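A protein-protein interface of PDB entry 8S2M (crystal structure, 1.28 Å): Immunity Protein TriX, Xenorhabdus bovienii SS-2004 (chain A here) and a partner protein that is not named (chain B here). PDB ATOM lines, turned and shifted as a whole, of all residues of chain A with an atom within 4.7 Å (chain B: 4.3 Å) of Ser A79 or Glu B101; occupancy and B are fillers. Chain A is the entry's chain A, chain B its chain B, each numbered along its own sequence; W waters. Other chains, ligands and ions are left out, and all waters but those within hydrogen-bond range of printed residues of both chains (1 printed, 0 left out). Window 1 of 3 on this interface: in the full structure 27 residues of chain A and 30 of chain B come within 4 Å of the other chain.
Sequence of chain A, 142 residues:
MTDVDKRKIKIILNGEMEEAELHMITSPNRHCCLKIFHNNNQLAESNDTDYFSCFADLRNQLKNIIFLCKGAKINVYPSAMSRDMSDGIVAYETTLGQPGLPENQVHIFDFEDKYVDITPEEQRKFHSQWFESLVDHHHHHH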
ATOM      1  N   TYR A  77      28.679  13.815  -3.313  1.00  0.00           N
ATOM      2  CA  TYR A  77      27.357  14.430  -3.303  1.00  0.00           C
ATOM      3  C   TYR A  77      26.444  13.529  -2.492  1.00  0.00           C
ATOM      4  O   TYR A  77      26.613  12.311  -2.524  1.00  0.00           O
ATOM      5  CB  TYR A  77      26.812  14.591  -4.735  1.00  0.00           C
ATOM      6  CG  TYR A  77      26.077  15.894  -4.956  1.00  0.00           C
ATOM      7  CD1 TYR A  77      26.775  17.067  -5.201  1.00  0.00           C
ATOM      8  CD2 TYR A  77      24.681  15.950  -4.923  1.00  0.00           C
ATOM      9  CE1 TYR A  77      26.112  18.260  -5.403  1.00  0.00           C
ATOM     10  CE2 TYR A  77      24.007  17.144  -5.128  1.00  0.00           C
ATOM     11  CZ  TYR A  77      24.731  18.296  -5.362  1.00  0.00           C
ATOM     12  OH  TYR A  77      24.099  19.506  -5.553  1.00  0.00           O
ATOM     13  N   PRO A  78      25.482  14.079  -1.757  1.00  0.00           N
ATOM     14  CA  PRO A  78      24.526  13.209  -1.057  1.00  0.00           C
ATOM     15  C   PRO A  78      23.561  12.573  -2.042  1.00  0.00           C
ATOM     16  O   PRO A  78      23.243  13.157  -3.083  1.00  0.00           O
ATOM     17  CB  PRO A  78      23.753  14.175  -0.153  1.00  0.00           C
ATOM     18  CG  PRO A  78      24.457  15.472  -0.219  1.00  0.00           C
ATOM     19  CD  PRO A  78      25.228  15.504  -1.494  1.00  0.00           C
ATOM     20  N   SER A  79      23.073  11.378  -1.692  1.00  0.00           N
ATOM     21  CA  SER A  79      21.863  10.908  -2.345  1.00  0.00           C
ATOM     22  C   SER A  79      20.669  11.634  -1.733  1.00  0.00           C
ATOM     23  O   SER A  79      20.788  12.307  -0.698  1.00  0.00           O
ATOM     24  CB  SER A  79      21.714   9.403  -2.169  1.00  0.00           C
ATOM     25  OG  SER A  79      21.473   9.082  -0.809  1.00  0.00           O
ATOM     26  N   ALA A  80      19.499  11.492  -2.355  1.00  0.00           N
ATOM     27  CA  ALA A  80      18.290  12.040  -1.738  1.00  0.00           C
ATOM     28  C   ALA A  80      18.097  11.459  -0.349  1.00  0.00           C
ATOM     29  O   ALA A  80      17.820  12.185   0.617  1.00  0.00           O
ATOM     30  CB  ALA A  80      17.061  11.760  -2.597  1.00  0.00           C
ATOM     31  N   MET A  81      18.273  10.147  -0.237  1.00  0.00           N
ATOM     32  CA  MET A  81      18.098   9.477   1.045  1.00  0.00           C
ATOM     33  C   MET A  81      19.137   9.923   2.063  1.00  0.00           C
ATOM     34  O   MET A  81      18.810  10.140   3.237  1.00  0.00           O
ATOM     35  CB  MET A  81      18.159   7.959   0.857  1.00  0.00           C
ATOM     36  CG  MET A  81      17.861   7.218   2.135  1.00  0.00           C
ATOM     37  SD  MET A  81      17.843   5.422   1.997  1.00  0.00           S
ATOM     38  CE  MET A  81      16.608   5.176   0.746  1.00  0.00           C
ATOM     39  N   SER A  82      20.408   9.988   1.658  1.00  0.00           N
ATOM     40  CA  SER A  82      21.432  10.355   2.631  1.00  0.00           C
ATOM     41  C   SER A  82      21.254  11.797   3.075  1.00  0.00           C
ATOM     42  O   SER A  82      21.395  12.110   4.269  1.00  0.00           O
ATOM     43  CB  SER A  82      22.845  10.068   2.102  1.00  0.00           C
ATOM     44  OG  SER A  82      23.337  11.090   1.251  1.00  0.00           O
ATOM     45  N   ARG A  83      20.902  12.689   2.147  1.00  0.00           N
ATOM     46  CA  ARG A  83      20.624  14.066   2.534  1.00  0.00           C
ATOM     47  C   ARG A  83      19.478  14.118   3.538  1.00  0.00           C
ATOM     48  O   ARG A  83      19.579  14.751   4.600  1.00  0.00           O
ATOM     49  CB  ARG A  83      20.274  14.898   1.301  1.00  0.00           C
ATOM     50  CG  ARG A  83      20.120  16.373   1.632  1.00  0.00           C
ATOM     51  CD  ARG A  83      19.579  17.164   0.450  1.00  0.00           C
ATOM     52  NE  ARG A  83      20.418  17.067  -0.741  1.00  0.00           N
ATOM     53  CZ  ARG A  83      21.389  17.911  -1.061  1.00  0.00           C
ATOM     54  NH1 ARG A  83      21.740  18.911  -0.261  1.00  0.00           N
ATOM     55  NH2 ARG A  83      22.033  17.750  -2.218  1.00  0.00           N
ATOM     56  N   TYR A  92      28.089  10.494  -0.759  1.00  0.00           N
ATOM     57  CA  TYR A  92      28.736   9.418  -1.495  1.00  0.00           C
ATOM     58  C   TYR A  92      29.867   9.959  -2.360  1.00  0.00           C
ATOM     59  O   TYR A  92      29.742  11.021  -2.979  1.00  0.00           O
ATOM     60  CB  TYR A  92      27.746   8.780  -2.465  1.00  0.00           C
ATOM     61  CG  TYR A  92      26.692   7.893  -1.862  1.00  0.00           C
ATOM     62  CD1 TYR A  92      25.520   8.437  -1.338  1.00  0.00           C
ATOM     63  CD2 TYR A  92      26.847   6.515  -1.854  1.00  0.00           C
ATOM     64  CE1 TYR A  92      24.527   7.618  -0.819  1.00  0.00           C
ATOM     65  CE2 TYR A  92      25.868   5.683  -1.344  1.00  0.00           C
ATOM     66  CZ  TYR A  92      24.719   6.238  -0.830  1.00  0.00           C
ATOM     67  OH  TYR A  92      23.772   5.371  -0.343  1.00  0.00           O
ATOM     68  N   THR B  57      13.287   3.326   3.173  1.00  0.00           N
ATOM     69  CA  THR B  57      13.886   2.154   2.545  1.00  0.00           C
ATOM     70  C   THR B  57      13.152   0.888   2.956  1.00  0.00           C
ATOM     71  O   THR B  57      12.610   0.790   4.064  1.00  0.00           O
ATOM     72  CB  THR B  57      15.393   2.034   2.882  1.00  0.00           C
ATOM     73  OG1 THR B  57      15.920   0.822   2.325  1.00  0.00           O
ATOM     74  CG2 THR B  57      15.630   2.035   4.368  1.00  0.00           C
ATOM     75  N   LYS B  62      19.782  -0.362   5.827  1.00  0.00           N
ATOM     76  CA  LYS B  62      20.218   0.791   5.044  1.00  0.00           C
ATOM     77  C   LYS B  62      19.999   2.106   5.770  1.00  0.00           C
ATOM     78  O   LYS B  62      20.488   3.135   5.295  1.00  0.00           O
ATOM     79  CB  LYS B  62      19.511   0.832   3.685  1.00  0.00           C
ATOM     80  CG  LYS B  62      19.820  -0.352   2.797  1.00  0.00           C
ATOM     81  CD  LYS B  62      21.277  -0.404   2.414  1.00  0.00           C
ATOM     82  CE  LYS B  62      21.552  -1.657   1.602  1.00  0.00           C
ATOM     83  NZ  LYS B  62      22.855  -1.534   0.924  1.00  0.00           N
ATOM     84  N   PHE B  66      22.970   6.368   8.065  1.00  0.00           N
ATOM     85  CA  PHE B  66      22.400   7.711   8.029  1.00  0.00           C
ATOM     86  C   PHE B  66      21.928   8.147   9.413  1.00  0.00           C
ATOM     87  O   PHE B  66      22.190   9.283   9.831  1.00  0.00           O
ATOM     88  CB  PHE B  66      21.249   7.751   7.023  1.00  0.00           C
ATOM     89  CG  PHE B  66      21.645   7.346   5.627  1.00  0.00           C
ATOM     90  CD1 PHE B  66      22.923   7.589   5.132  1.00  0.00           C
ATOM     91  CD2 PHE B  66      20.732   6.701   4.815  1.00  0.00           C
ATOM     92  CE1 PHE B  66      23.278   7.192   3.844  1.00  0.00           C
ATOM     93  CE2 PHE B  66      21.079   6.320   3.519  1.00  0.00           C
ATOM     94  CZ  PHE B  66      22.345   6.560   3.040  1.00  0.00           C
ATOM     95  N   PHE B  98      21.303   5.539  -6.752  1.00  0.00           N
ATOM     96  CA  PHE B  98      21.734   4.862  -5.533  1.00  0.00           C
ATOM     97  C   PHE B  98      20.835   3.668  -5.280  1.00  0.00           C
ATOM     98  O   PHE B  98      20.243   3.507  -4.209  1.00  0.00           O
ATOM     99  CB  PHE B  98      21.776   5.853  -4.369  1.00  0.00           C
ATOM    100  CG  PHE B  98      22.656   7.044  -4.639  1.00  0.00           C
ATOM    101  CD1 PHE B  98      24.035   6.972  -4.442  1.00  0.00           C
ATOM    102  CD2 PHE B  98      22.114   8.212  -5.150  1.00  0.00           C
ATOM    103  CE1 PHE B  98      24.844   8.060  -4.709  1.00  0.00           C
ATOM    104  CE2 PHE B  98      22.918   9.301  -5.416  1.00  0.00           C
ATOM    105  CZ  PHE B  98      24.279   9.232  -5.199  1.00  0.00           C
ATOM    106  N   ALA B  99      20.738   2.804  -6.296  1.00  0.00           N
ATOM    107  CA  ALA B  99      19.772   1.709  -6.300  1.00  0.00           C
ATOM    108  C   ALA B  99      19.924   0.786  -5.097  1.00  0.00           C
ATOM    109  O   ALA B  99      18.939   0.188  -4.651  1.00  0.00           O
ATOM    110  CB  ALA B  99      19.912   0.913  -7.597  1.00  0.00           C
ATOM    111  N   ALA B 100      21.142   0.652  -4.567  1.00  0.00           N
ATOM    112  CA  ALA B 100      21.359  -0.235  -3.429  1.00  0.00           C
ATOM    113  C   ALA B 100      20.591   0.204  -2.186  1.00  0.00           C
ATOM    114  O   ALA B 100      20.392  -0.604  -1.271  1.00  0.00           O
ATOM    115  CB  ALA B 100      22.853  -0.359  -3.126  1.00  0.00           C
ATOM    116  N   GLU B 101      20.142   1.456  -2.135  1.00  0.00           N
ATOM    117  CA  GLU B 101      19.418   1.967  -0.978  1.00  0.00           C
ATOM    118  C   GLU B 101      18.008   1.397  -0.863  1.00  0.00           C
ATOM    119  O   GLU B 101      17.394   1.528   0.202  1.00  0.00           O
ATOM    120  CB  GLU B 101      19.305   3.483  -1.079  1.00  0.00           C
ATOM    121  CG  GLU B 101      20.631   4.196  -0.917  1.00  0.00           C
ATOM    122  CD  GLU B 101      20.508   5.689  -1.104  1.00  0.00           C
ATOM    123  OE1 GLU B 101      19.524   6.144  -1.744  1.00  0.00           O
ATOM    124  OE2 GLU B 101      21.398   6.409  -0.607  1.00  0.00           O
ATOM    125  N   ALA B 102      17.469   0.795  -1.925  1.00  0.00           N
ATOM    126  CA  ALA B 102      16.110   0.241  -1.919  1.00  0.00           C
ATOM    127  C   ALA B 102      15.072   1.276  -1.469  1.00  0.00           C
ATOM    128  O   ALA B 102      14.258   1.038  -0.572  1.00  0.00           O
ATOM    129  CB  ALA B 102      16.035  -1.045  -1.099  1.00  0.00           C
ATOM    130  N   GLU B 103      15.084   2.423  -2.141  1.00  0.00           N
ATOM    131  CA  GLU B 103      14.303   3.583  -1.726  1.00  0.00           C
ATOM    132  C   GLU B 103      12.839   3.500  -2.148  1.00  0.00           C
ATOM    133  O   GLU B 103      12.521   3.235  -3.319  1.00  0.00           O
ATOM    134  CB  GLU B 103      14.925   4.859  -2.295  1.00  0.00           C
ATOM    135  CG  GLU B 103      14.240   6.144  -1.846  1.00  0.00           C
ATOM    136  CD  GLU B 103      14.905   7.411  -2.384  1.00  0.00           C
ATOM    137  OE1 GLU B 103      15.828   7.324  -3.222  1.00  0.00           O
ATOM    138  OE2 GLU B 103      14.472   8.521  -1.994  1.00  0.00           O
HETATM  139  O   HOH W   1      18.400   8.481  -2.500  1.00  0.00           O
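OE2 of Glu B101 sits at hydrogen-bond distance from OG of Ser A79, 2.7 Å away.
The side-chain hydroxyl of Tyr A92 sits at hydrogen-bond distance from the side-chain carboxylate of Glu B101.
The backbone carbonyl oxygen (O) of Tyr A77 lies within hydrogen-bond range of the backbone NH (N) of Tyr A92, at 2.9 Å.
N of Met A81 sits close to OG of Ser A79, at 3.4 Å.
The side-chain hydroxyl (OG) of Ser A79 sits at hydrogen-bond distance from the backbone NH (N) of Ser A82.
OG1 of Thr B57 lies within hydrogen-bond range of O of Glu B101 (2.7 Å).
The side-chain hydroxyl of Thr B57 sits close to the backbone carbonyl oxygen of Ala B102 (3.3 Å).
Ser A79 touches Phe B98.
Thr B57 touches Met A81.
Phe B66 touches Met A81 (CE2 to CG, 3.6 Å).
Met A81 touches Glu B101 (CB to OE1, 3.5 Å).
CE of Met A81 touches CB of Glu B103, at 3.5 Å.
Ser A82 touches Phe B66.
Tyr A92 touches Phe B66.
Tyr A92 touches Phe B98.
Of chain B, only Phe B98 (3.2 Å) and Glu B101 (2.7 Å) come within 4 Å of Ser A79.
Of chain A, only Ser A79, Met A81 and Tyr A92 come within 4 Å of Glu B101.
Of the printed residues of chain A, Glu B103 touches Met A81.
Of the printed residues of chain B, Ser A82 touches Phe B66.
Of the printed residues of chain B, Met A81 touches Thr B57 (3.99 Å), Phe B66 (3.6 Å), Glu B101 (3.5 Å) and Glu B103 (3.5 Å).
Printed residues of chain B within 4 Å of Tyr A92: Phe B66 (3.9 Å), Phe B98 (3.4 Å) and Glu B101 (2.6 Å).
Ala A80 touches none of the printed residues of chain B.
Ala B100 touches none of the printed residues of chain A.
The nearest printed residue of chain B that does not touch Ser A79 is Phe B66 (4.7 Å).
The nearest printed residue of chain A that does not touch Glu B103 is Ala A80 (4.2 Å).
Of the 8 printed residues of chain A, 4 touch a printed residue of chain B.
Of the 9 printed residues of chain B, 5 touch a printed residue of chain A.
Hydrophobic or aromatic side chains of chain B within 4 Å of the printed part of chain A: Phe B66 and Phe B98.
Water W1 lies within hydrogen-bond range of OE1 of Glu B101 (2.7 Å), N of Met A81 (2.8 Å), OE1 of Glu B103 (2.9 Å) and N of Ala A80 (3.2 Å).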
